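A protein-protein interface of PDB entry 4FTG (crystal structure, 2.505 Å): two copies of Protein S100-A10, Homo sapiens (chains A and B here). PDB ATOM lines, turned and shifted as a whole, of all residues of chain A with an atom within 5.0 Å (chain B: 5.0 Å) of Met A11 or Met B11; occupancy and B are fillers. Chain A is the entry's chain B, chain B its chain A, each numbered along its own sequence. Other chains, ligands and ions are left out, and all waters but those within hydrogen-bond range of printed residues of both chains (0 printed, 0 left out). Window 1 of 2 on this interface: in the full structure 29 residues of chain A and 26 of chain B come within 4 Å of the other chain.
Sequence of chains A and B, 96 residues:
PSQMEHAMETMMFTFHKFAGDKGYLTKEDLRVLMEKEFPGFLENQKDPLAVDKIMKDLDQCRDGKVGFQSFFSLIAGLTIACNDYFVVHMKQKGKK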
ATOM      1  N   MET A   4       0.034 -22.596   9.127  1.00  0.00           N
ATOM      2  CA  MET A   4       0.534 -21.225   9.247  1.00  0.00           C
ATOM      3  C   MET A   4      -0.020 -20.349   8.148  1.00  0.00           C
ATOM      4  O   MET A   4      -0.411 -19.198   8.379  1.00  0.00           O
ATOM      5  CB  MET A   4       2.065 -21.195   9.198  1.00  0.00           C
ATOM      6  CG  MET A   4       2.766 -21.555  10.509  1.00  0.00           C
ATOM      7  SD  MET A   4       2.340 -20.568  11.994  1.00  0.00           S
ATOM      8  CE  MET A   4       2.701 -18.879  11.526  1.00  0.00           C
ATOM      9  N   ALA A   7      -3.477 -19.501   9.118  1.00  0.00           N
ATOM     10  CA  ALA A   7      -3.395 -18.534  10.198  1.00  0.00           C
ATOM     11  C   ALA A   7      -3.125 -17.139   9.643  1.00  0.00           C
ATOM     12  O   ALA A   7      -3.786 -16.146  10.018  1.00  0.00           O
ATOM     13  CB  ALA A   7      -2.311 -18.953  11.166  1.00  0.00           C
ATOM     14  N   MET A   8      -2.166 -17.061   8.728  1.00  0.00           N
ATOM     15  CA  MET A   8      -1.766 -15.760   8.212  1.00  0.00           C
ATOM     16  C   MET A   8      -2.907 -15.169   7.439  1.00  0.00           C
ATOM     17  O   MET A   8      -3.280 -14.015   7.661  1.00  0.00           O
ATOM     18  CB  MET A   8      -0.514 -15.885   7.370  1.00  0.00           C
ATOM     19  CG  MET A   8       0.720 -16.216   8.193  1.00  0.00           C
ATOM     20  SD  MET A   8       1.997 -16.944   7.154  1.00  0.00           S
ATOM     21  CE  MET A   8       2.420 -15.524   6.120  1.00  0.00           C
ATOM     22  N   GLU A   9      -3.515 -15.983   6.579  1.00  0.00           N
ATOM     23  CA  GLU A   9      -4.669 -15.532   5.792  1.00  0.00           C
ATOM     24  C   GLU A   9      -5.823 -15.058   6.675  1.00  0.00           C
ATOM     25  O   GLU A   9      -6.485 -14.073   6.376  1.00  0.00           O
ATOM     26  CB  GLU A   9      -5.143 -16.650   4.862  1.00  0.00           C
ATOM     27  CG  GLU A   9      -6.295 -16.265   3.949  1.00  0.00           C
ATOM     28  CD  GLU A   9      -6.387 -17.161   2.718  1.00  0.00           C
ATOM     29  OE1 GLU A   9      -5.337 -17.395   2.051  1.00  0.00           O
ATOM     30  OE2 GLU A   9      -7.509 -17.624   2.412  1.00  0.00           O
ATOM     31  N   THR A  10      -6.047 -15.758   7.773  1.00  0.00           N
ATOM     32  CA  THR A  10      -7.070 -15.367   8.742  1.00  0.00           C
ATOM     33  C   THR A  10      -6.850 -13.984   9.363  1.00  0.00           C
ATOM     34  O   THR A  10      -7.760 -13.156   9.415  1.00  0.00           O
ATOM     35  CB  THR A  10      -7.213 -16.437   9.844  1.00  0.00           C
ATOM     36  OG1 THR A  10      -7.840 -17.593   9.279  1.00  0.00           O
ATOM     37  CG2 THR A  10      -8.060 -15.904  11.018  1.00  0.00           C
ATOM     38  N   MET A  11      -5.642 -13.736   9.835  1.00  0.00           N
ATOM     39  CA  MET A  11      -5.293 -12.418  10.345  1.00  0.00           C
ATOM     40  C   MET A  11      -5.492 -11.340   9.295  1.00  0.00           C
ATOM     41  O   MET A  11      -6.058 -10.266   9.572  1.00  0.00           O
ATOM     42  CB  MET A  11      -3.853 -12.444  10.814  1.00  0.00           C
ATOM     43  CG  MET A  11      -3.619 -13.565  11.830  1.00  0.00           C
ATOM     44  SD  MET A  11      -2.233 -13.250  12.930  1.00  0.00           S
ATOM     45  CE  MET A  11      -2.530 -14.496  14.182  1.00  0.00           C
ATOM     46  N   MET A  12      -5.045 -11.649   8.083  1.00  0.00           N
ATOM     47  CA  MET A  12      -5.141 -10.720   6.964  1.00  0.00           C
ATOM     48  C   MET A  12      -6.599 -10.463   6.654  1.00  0.00           C
ATOM     49  O   MET A  12      -7.016  -9.312   6.463  1.00  0.00           O
ATOM     50  CB  MET A  12      -4.445 -11.303   5.741  1.00  0.00           C
ATOM     51  CG  MET A  12      -3.928 -10.297   4.732  1.00  0.00           C
ATOM     52  SD  MET A  12      -3.073 -11.134   3.361  1.00  0.00           S
ATOM     53  CE  MET A  12      -4.421 -11.458   2.257  1.00  0.00           C
ATOM     54  N   PHE A  13      -7.395 -11.527   6.633  1.00  0.00           N
ATOM     55  CA  PHE A  13      -8.826 -11.368   6.319  1.00  0.00           C
ATOM     56  C   PHE A  13      -9.611 -10.687   7.453  1.00  0.00           C
ATOM     57  O   PHE A  13     -10.511  -9.876   7.201  1.00  0.00           O
ATOM     58  CB  PHE A  13      -9.464 -12.692   5.873  1.00  0.00           C
ATOM     59  CG  PHE A  13      -9.076 -13.116   4.454  1.00  0.00           C
ATOM     60  CD1 PHE A  13      -8.256 -12.306   3.662  1.00  0.00           C
ATOM     61  CD2 PHE A  13      -9.543 -14.318   3.906  1.00  0.00           C
ATOM     62  CE1 PHE A  13      -7.904 -12.691   2.358  1.00  0.00           C
ATOM     63  CE2 PHE A  13      -9.196 -14.709   2.605  1.00  0.00           C
ATOM     64  CZ  PHE A  13      -8.373 -13.894   1.833  1.00  0.00           C
ATOM     65  N   THR A  14      -9.256 -10.996   8.699  1.00  0.00           N
ATOM     66  CA  THR A  14      -9.855 -10.306   9.834  1.00  0.00           C
ATOM     67  C   THR A  14      -9.588  -8.799   9.773  1.00  0.00           C
ATOM     68  O   THR A  14     -10.485  -8.020  10.008  1.00  0.00           O
ATOM     69  CB  THR A  14      -9.333 -10.826  11.173  1.00  0.00           C
ATOM     70  OG1 THR A  14      -9.657 -12.207  11.310  1.00  0.00           O
ATOM     71  CG2 THR A  14      -9.954 -10.046  12.304  1.00  0.00           C
ATOM     72  N   PHE A  15      -8.370  -8.384   9.431  1.00  0.00           N
ATOM     73  CA  PHE A  15      -8.099  -6.948   9.349  1.00  0.00           C
ATOM     74  C   PHE A  15      -9.029  -6.286   8.351  1.00  0.00           C
ATOM     75  O   PHE A  15      -9.708  -5.309   8.675  1.00  0.00           O
ATOM     76  CB  PHE A  15      -6.656  -6.653   8.961  1.00  0.00           C
ATOM     77  CG  PHE A  15      -6.373  -5.171   8.720  1.00  0.00           C
ATOM     78  CD1 PHE A  15      -6.316  -4.657   7.419  1.00  0.00           C
ATOM     79  CD2 PHE A  15      -6.156  -4.302   9.787  1.00  0.00           C
ATOM     80  CE1 PHE A  15      -6.055  -3.307   7.176  1.00  0.00           C
ATOM     81  CE2 PHE A  15      -5.881  -2.940   9.551  1.00  0.00           C
ATOM     82  CZ  PHE A  15      -5.833  -2.445   8.245  1.00  0.00           C
ATOM     83  N   PHE A  68      -2.511  -2.136   8.782  1.00  0.00           N
ATOM     84  CA  PHE A  68      -2.329  -3.562   8.979  1.00  0.00           C
ATOM     85  C   PHE A  68      -1.126  -3.880   9.837  1.00  0.00           C
ATOM     86  O   PHE A  68      -1.173  -4.755  10.702  1.00  0.00           O
ATOM     87  CB  PHE A  68      -2.185  -4.294   7.657  1.00  0.00           C
ATOM     88  CG  PHE A  68      -2.069  -5.774   7.819  1.00  0.00           C
ATOM     89  CD1 PHE A  68      -3.120  -6.503   8.362  1.00  0.00           C
ATOM     90  CD2 PHE A  68      -0.931  -6.434   7.457  1.00  0.00           C
ATOM     91  CE1 PHE A  68      -3.030  -7.870   8.523  1.00  0.00           C
ATOM     92  CE2 PHE A  68      -0.829  -7.811   7.613  1.00  0.00           C
ATOM     93  CZ  PHE A  68      -1.879  -8.526   8.146  1.00  0.00           C
ATOM     94  N   PHE A  71      -1.870  -3.140  13.318  1.00  0.00           N
ATOM     95  CA  PHE A  71      -2.776  -4.215  13.707  1.00  0.00           C
ATOM     96  C   PHE A  71      -2.001  -5.480  14.077  1.00  0.00           C
ATOM     97  O   PHE A  71      -2.317  -6.151  15.064  1.00  0.00           O
ATOM     98  CB  PHE A  71      -3.779  -4.532  12.589  1.00  0.00           C
ATOM     99  CG  PHE A  71      -4.571  -5.769  12.844  1.00  0.00           C
ATOM    100  CD1 PHE A  71      -5.517  -5.801  13.839  1.00  0.00           C
ATOM    101  CD2 PHE A  71      -4.343  -6.919  12.115  1.00  0.00           C
ATOM    102  CE1 PHE A  71      -6.234  -6.965  14.094  1.00  0.00           C
ATOM    103  CE2 PHE A  71      -5.057  -8.070  12.368  1.00  0.00           C
ATOM    104  CZ  PHE A  71      -5.997  -8.092  13.359  1.00  0.00           C
ATOM    105  N   PHE A  72      -0.977  -5.791  13.288  1.00  0.00           N
ATOM    106  CA  PHE A  72      -0.180  -6.986  13.518  1.00  0.00           C
ATOM    107  C   PHE A  72       0.639  -6.884  14.798  1.00  0.00           C
ATOM    108  O   PHE A  72       0.921  -7.887  15.454  1.00  0.00           O
ATOM    109  CB  PHE A  72       0.737  -7.283  12.334  1.00  0.00           C
ATOM    110  CG  PHE A  72       1.110  -8.712  12.240  1.00  0.00           C
ATOM    111  CD1 PHE A  72       0.268  -9.613  11.606  1.00  0.00           C
ATOM    112  CD2 PHE A  72       2.283  -9.177  12.821  1.00  0.00           C
ATOM    113  CE1 PHE A  72       0.577 -10.941  11.559  1.00  0.00           C
ATOM    114  CE2 PHE A  72       2.613 -10.515  12.759  1.00  0.00           C
ATOM    115  CZ  PHE A  72       1.757 -11.398  12.129  1.00  0.00           C
ATOM    116  N   ILE A  75      -1.762  -8.010  17.643  1.00  0.00           N
ATOM    117  CA  ILE A  75      -1.853  -9.450  17.696  1.00  0.00           C
ATOM    118  C   ILE A  75      -0.551 -10.049  18.211  1.00  0.00           C
ATOM    119  O   ILE A  75      -0.558 -11.003  18.998  1.00  0.00           O
ATOM    120  CB  ILE A  75      -2.167 -10.003  16.316  1.00  0.00           C
ATOM    121  CG1 ILE A  75      -3.527  -9.474  15.867  1.00  0.00           C
ATOM    122  CG2 ILE A  75      -2.150 -11.509  16.352  1.00  0.00           C
ATOM    123  CD1 ILE A  75      -4.588  -9.501  16.980  1.00  0.00           C
ATOM    124  N   THR A  79      -0.266 -12.457  21.539  1.00  0.00           N
ATOM    125  CA  THR A  79       0.185 -13.818  21.344  1.00  0.00           C
ATOM    126  C   THR A  79       1.464 -14.050  22.116  1.00  0.00           C
ATOM    127  O   THR A  79       1.693 -15.132  22.645  1.00  0.00           O
ATOM    128  CB  THR A  79       0.413 -14.106  19.854  1.00  0.00           C
ATOM    129  OG1 THR A  79      -0.789 -13.818  19.144  1.00  0.00           O
ATOM    130  CG2 THR A  79       0.789 -15.565  19.618  1.00  0.00           C
ATOM    131  N   MET B   4      -9.565 -15.282  15.163  1.00  0.00           N
ATOM    132  CA  MET B   4      -8.264 -14.759  15.606  1.00  0.00           C
ATOM    133  C   MET B   4      -7.621 -15.639  16.683  1.00  0.00           C
ATOM    134  O   MET B   4      -6.417 -15.906  16.648  1.00  0.00           O
ATOM    135  CB  MET B   4      -8.384 -13.311  16.090  1.00  0.00           C
ATOM    136  CG  MET B   4      -8.468 -12.266  14.957  1.00  0.00           C
ATOM    137  SD  MET B   4      -7.159 -12.471  13.712  1.00  0.00           S
ATOM    138  CE  MET B   4      -5.693 -11.925  14.588  1.00  0.00           C
ATOM    139  N   ALA B   7      -6.194 -18.795  14.915  1.00  0.00           N
ATOM    140  CA  ALA B   7      -4.993 -18.406  14.199  1.00  0.00           C
ATOM    141  C   ALA B   7      -3.821 -18.169  15.158  1.00  0.00           C
ATOM    142  O   ALA B   7      -2.728 -18.702  14.926  1.00  0.00           O
ATOM    143  CB  ALA B   7      -5.266 -17.159  13.365  1.00  0.00           C
ATOM    144  N   MET B   8      -4.044 -17.392  16.230  1.00  0.00           N
ATOM    145  CA  MET B   8      -2.988 -17.150  17.237  1.00  0.00           C
ATOM    146  C   MET B   8      -2.439 -18.431  17.849  1.00  0.00           C
ATOM    147  O   MET B   8      -1.211 -18.636  17.935  1.00  0.00           O
ATOM    148  CB  MET B   8      -3.470 -16.213  18.340  1.00  0.00           C
ATOM    149  CG  MET B   8      -3.655 -14.812  17.866  1.00  0.00           C
ATOM    150  SD  MET B   8      -4.853 -13.861  18.826  1.00  0.00           S
ATOM    151  CE  MET B   8      -3.906 -13.579  20.315  1.00  0.00           C
ATOM    152  N   GLU B   9      -3.340 -19.316  18.239  1.00  0.00           N
ATOM    153  CA  GLU B   9      -2.911 -20.579  18.817  1.00  0.00           C
ATOM    154  C   GLU B   9      -2.057 -21.398  17.864  1.00  0.00           C
ATOM    155  O   GLU B   9      -1.070 -22.022  18.312  1.00  0.00           O
ATOM    156  CB  GLU B   9      -4.108 -21.396  19.275  1.00  0.00           C
ATOM    157  CG  GLU B   9      -3.722 -22.763  19.835  1.00  0.00           C
ATOM    158  CD  GLU B   9      -4.748 -23.281  20.792  1.00  0.00           C
ATOM    159  OE1 GLU B   9      -5.146 -22.496  21.681  1.00  0.00           O
ATOM    160  OE2 GLU B   9      -5.178 -24.451  20.643  1.00  0.00           O
ATOM    161  N   THR B  10      -2.417 -21.411  16.566  1.00  0.00           N
ATOM    162  CA  THR B  10      -1.653 -22.250  15.640  1.00  0.00           C
ATOM    163  C   THR B  10      -0.270 -21.667  15.498  1.00  0.00           C
ATOM    164  O   THR B  10       0.713 -22.402  15.394  1.00  0.00           O
ATOM    165  CB  THR B  10      -2.342 -22.606  14.265  1.00  0.00           C
ATOM    166  OG1 THR B  10      -1.791 -21.835  13.205  1.00  0.00           O
ATOM    167  CG2 THR B  10      -3.807 -22.432  14.304  1.00  0.00           C
ATOM    168  N   MET B  11      -0.186 -20.347  15.567  1.00  0.00           N
ATOM    169  CA  MET B  11       1.117 -19.693  15.584  1.00  0.00           C
ATOM    170  C   MET B  11       1.912 -20.047  16.836  1.00  0.00           C
ATOM    171  O   MET B  11       3.095 -20.365  16.752  1.00  0.00           O
ATOM    172  CB  MET B  11       0.989 -18.179  15.394  1.00  0.00           C
ATOM    173  CG  MET B  11       0.408 -17.823  14.039  1.00  0.00           C
ATOM    174  SD  MET B  11       0.670 -16.089  13.572  1.00  0.00           S
ATOM    175  CE  MET B  11       2.411 -16.056  13.936  1.00  0.00           C
ATOM    176  N   MET B  12       1.250 -20.034  17.987  1.00  0.00           N
ATOM    177  CA  MET B  12       1.902 -20.459  19.221  1.00  0.00           C
ATOM    178  C   MET B  12       2.379 -21.893  19.125  1.00  0.00           C
ATOM    179  O   MET B  12       3.541 -22.204  19.393  1.00  0.00           O
ATOM    180  CB  MET B  12       0.949 -20.337  20.407  1.00  0.00           C
ATOM    181  CG  MET B  12       1.668 -20.321  21.752  1.00  0.00           C
ATOM    182  SD  MET B  12       0.673 -19.622  23.087  1.00  0.00           S
ATOM    183  CE  MET B  12      -0.268 -21.092  23.550  1.00  0.00           C
ATOM    184  N   PHE B  13       1.476 -22.773  18.722  1.00  0.00           N
ATOM    185  CA  PHE B  13       1.789 -24.199  18.706  1.00  0.00           C
ATOM    186  C   PHE B  13       2.813 -24.611  17.661  1.00  0.00           C
ATOM    187  O   PHE B  13       3.594 -25.529  17.894  1.00  0.00           O
ATOM    188  CB  PHE B  13       0.511 -25.018  18.603  1.00  0.00           C
ATOM    189  CG  PHE B  13      -0.262 -25.048  19.886  1.00  0.00           C
ATOM    190  CD1 PHE B  13       0.239 -24.408  21.014  1.00  0.00           C
ATOM    191  CD2 PHE B  13      -1.464 -25.718  19.983  1.00  0.00           C
ATOM    192  CE1 PHE B  13      -0.439 -24.439  22.223  1.00  0.00           C
ATOM    193  CE2 PHE B  13      -2.159 -25.749  21.190  1.00  0.00           C
ATOM    194  CZ  PHE B  13      -1.637 -25.107  22.320  1.00  0.00           C
ATOM    195  N   THR B  14       2.814 -23.908  16.529  1.00  0.00           N
ATOM    196  CA  THR B  14       3.768 -24.154  15.456  1.00  0.00           C
ATOM    197  C   THR B  14       5.181 -23.907  15.964  1.00  0.00           C
ATOM    198  O   THR B  14       6.094 -24.710  15.719  1.00  0.00           O
ATOM    199  CB  THR B  14       3.492 -23.228  14.248  1.00  0.00           C
ATOM    200  OG1 THR B  14       2.223 -23.558  13.661  1.00  0.00           O
ATOM    201  CG2 THR B  14       4.599 -23.350  13.205  1.00  0.00           C
ATOM    202  N   PHE B  15       5.353 -22.795  16.679  1.00  0.00           N
ATOM    203  CA  PHE B  15       6.632 -22.491  17.304  1.00  0.00           C
ATOM    204  C   PHE B  15       7.098 -23.673  18.123  1.00  0.00           C
ATOM    205  O   PHE B  15       8.220 -24.164  17.953  1.00  0.00           O
ATOM    206  CB  PHE B  15       6.557 -21.266  18.230  1.00  0.00           C
ATOM    207  CG  PHE B  15       7.880 -20.938  18.889  1.00  0.00           C
ATOM    208  CD1 PHE B  15       8.938 -20.401  18.137  1.00  0.00           C
ATOM    209  CD2 PHE B  15       8.093 -21.208  20.234  1.00  0.00           C
ATOM    210  CE1 PHE B  15      10.187 -20.110  18.721  1.00  0.00           C
ATOM    211  CE2 PHE B  15       9.338 -20.918  20.839  1.00  0.00           C
ATOM    212  CZ  PHE B  15      10.383 -20.372  20.079  1.00  0.00           C
ATOM    213  N   PHE B  68      10.360 -16.865  20.530  1.00  0.00           N
ATOM    214  CA  PHE B  68       9.022 -16.729  20.021  1.00  0.00           C
ATOM    215  C   PHE B  68       8.808 -15.345  19.436  1.00  0.00           C
ATOM    216  O   PHE B  68       8.244 -15.196  18.358  1.00  0.00           O
ATOM    217  CB  PHE B  68       7.985 -17.065  21.098  1.00  0.00           C
ATOM    218  CG  PHE B  68       6.585 -17.031  20.586  1.00  0.00           C
ATOM    219  CD1 PHE B  68       6.198 -17.874  19.566  1.00  0.00           C
ATOM    220  CD2 PHE B  68       5.671 -16.134  21.082  1.00  0.00           C
ATOM    221  CE1 PHE B  68       4.920 -17.831  19.061  1.00  0.00           C
ATOM    222  CE2 PHE B  68       4.392 -16.091  20.576  1.00  0.00           C
ATOM    223  CZ  PHE B  68       4.020 -16.949  19.565  1.00  0.00           C
ATOM    224  N   PHE B  71      10.438 -15.235  16.232  1.00  0.00           N
ATOM    225  CA  PHE B  71       9.623 -16.032  15.345  1.00  0.00           C
ATOM    226  C   PHE B  71       8.476 -15.179  14.798  1.00  0.00           C
ATOM    227  O   PHE B  71       8.239 -15.101  13.587  1.00  0.00           O
ATOM    228  CB  PHE B  71       9.085 -17.236  16.117  1.00  0.00           C
ATOM    229  CG  PHE B  71       7.991 -17.974  15.409  1.00  0.00           C
ATOM    230  CD1 PHE B  71       8.240 -18.629  14.205  1.00  0.00           C
ATOM    231  CD2 PHE B  71       6.716 -18.032  15.955  1.00  0.00           C
ATOM    232  CE1 PHE B  71       7.232 -19.323  13.549  1.00  0.00           C
ATOM    233  CE2 PHE B  71       5.692 -18.727  15.305  1.00  0.00           C
ATOM    234  CZ  PHE B  71       5.956 -19.369  14.100  1.00  0.00           C
ATOM    235  N   PHE B  72       7.787 -14.511  15.708  1.00  0.00           N
ATOM    236  CA  PHE B  72       6.671 -13.668  15.331  1.00  0.00           C
ATOM    237  C   PHE B  72       7.086 -12.506  14.428  1.00  0.00           C
ATOM    238  O   PHE B  72       6.310 -12.050  13.592  1.00  0.00           O
ATOM    239  CB  PHE B  72       5.952 -13.153  16.570  1.00  0.00           C
ATOM    240  CG  PHE B  72       4.489 -13.129  16.408  1.00  0.00           C
ATOM    241  CD1 PHE B  72       3.729 -14.214  16.789  1.00  0.00           C
ATOM    242  CD2 PHE B  72       3.867 -12.044  15.819  1.00  0.00           C
ATOM    243  CE1 PHE B  72       2.359 -14.206  16.626  1.00  0.00           C
ATOM    244  CE2 PHE B  72       2.495 -12.032  15.638  1.00  0.00           C
ATOM    245  CZ  PHE B  72       1.740 -13.122  16.042  1.00  0.00           C
ATOM    246  N   ILE B  75       7.064 -14.079  10.965  1.00  0.00           N
ATOM    247  CA  ILE B  75       5.707 -14.196  10.460  1.00  0.00           C
ATOM    248  C   ILE B  75       5.152 -12.820  10.099  1.00  0.00           C
ATOM    249  O   ILE B  75       4.423 -12.668   9.123  1.00  0.00           O
ATOM    250  CB  ILE B  75       4.766 -14.804  11.498  1.00  0.00           C
ATOM    251  CG1 ILE B  75       5.340 -16.103  12.072  1.00  0.00           C
ATOM    252  CG2 ILE B  75       3.385 -15.024  10.862  1.00  0.00           C
ATOM    253  CD1 ILE B  75       5.742 -17.121  11.006  1.00  0.00           C
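Met A11 touches just these residues of chain B: Met B4, Ala B7, Met B8 and Met B11.
Of the printed residues of chain A, Ile B75 touches Met A4 and Met A8.
Of the printed residues of chain A, Met B8 touches Met A11, Ile A75 and Thr A79.
Printed residues of chain A within 4 Å of Phe B68: Thr A79 (3.5 Å).
Of the printed residues of chain B, Thr A14 touches Met B4 (3.5 Å).
Of the printed residues of chain B, Ile A75 touches Met B4 (3.5 Å) and Met B8 (3.9 Å).
Phe B71 touches none of the printed residues of chain A.
The nearest printed residue of chain A that does not touch Met B8 is Ala A7 (5.6 Å).
O of Ile A75 sits at hydrogen-bond distance from OG1 of Thr A79, 2.8 Å away.
OG1 of Thr B14 sits at hydrogen-bond distance from O of Thr B10 (2.6 Å).
The backbone carbonyl oxygen of Thr A10 is in hydrogen-bond range of the side-chain hydroxyl of Thr A14.
CG of Met B11 touches CE of Met A4 (3.6 Å).
CE of Met A4 touches CD1 of Ile B75, at 3.6 Å.
Ala A7 touches Ala B7 (CB to O, 3.8 Å).
OG1 of Thr B10 touches CB of Ala A7 (3.6 Å).
Met A11 touches Met B4 (CG to CE, 3.8 Å).
Met B8 touches Met A11 (N to CE, 3.9 Å).
Met A11 touches Met B11.
Met B8 touches Ile A75 (CG to CG2, 3.9 Å).
Thr A79 touches Phe B68.
CG2 of Thr A79 touches CE1 of Phe B72 (3.6 Å).
Of the 14 printed residues of chain B, 9 touch a printed residue of chain A.
Hydrophobic or aromatic side chains of chain B that line the printed part of chain A: Met B4, Ala B7, Met B8, Met B11, Phe B68, Phe B72 and Ile B75.
Among the printed residues, 18 pairs touch across the chains.
Met A4 touches Met B11, and with the chains exchanged Met A11 touches Met B4.
Met A4 touches Thr B14, and with the chains exchanged Thr A14 touches Met B4.
Met A8 touches Ile B75, and with the chains exchanged Ile A75 touches Met B8.
Met A11 touches Met B8, but with the chains exchanged Met A8 does not touch Met B11 (5.4 Å).
Positions printed for both chains: 4, 7, 8, 9, 10, 11, 12, 13, 14, 15, 68, 71, 72 and 75.
Of the 18 pairs that touch across the chains among the printed residues, 13 have their exchanged pair printed and touching as well.
The side-chain hydroxyl (OG1) of Thr A14 lies within hydrogen-bond range of the side-chain sulfur (SD) of Met B4 (3.5 Å).
OG1 of Thr B14 is in hydrogen-bond range of SD of Met A4, 3.4 Å away.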
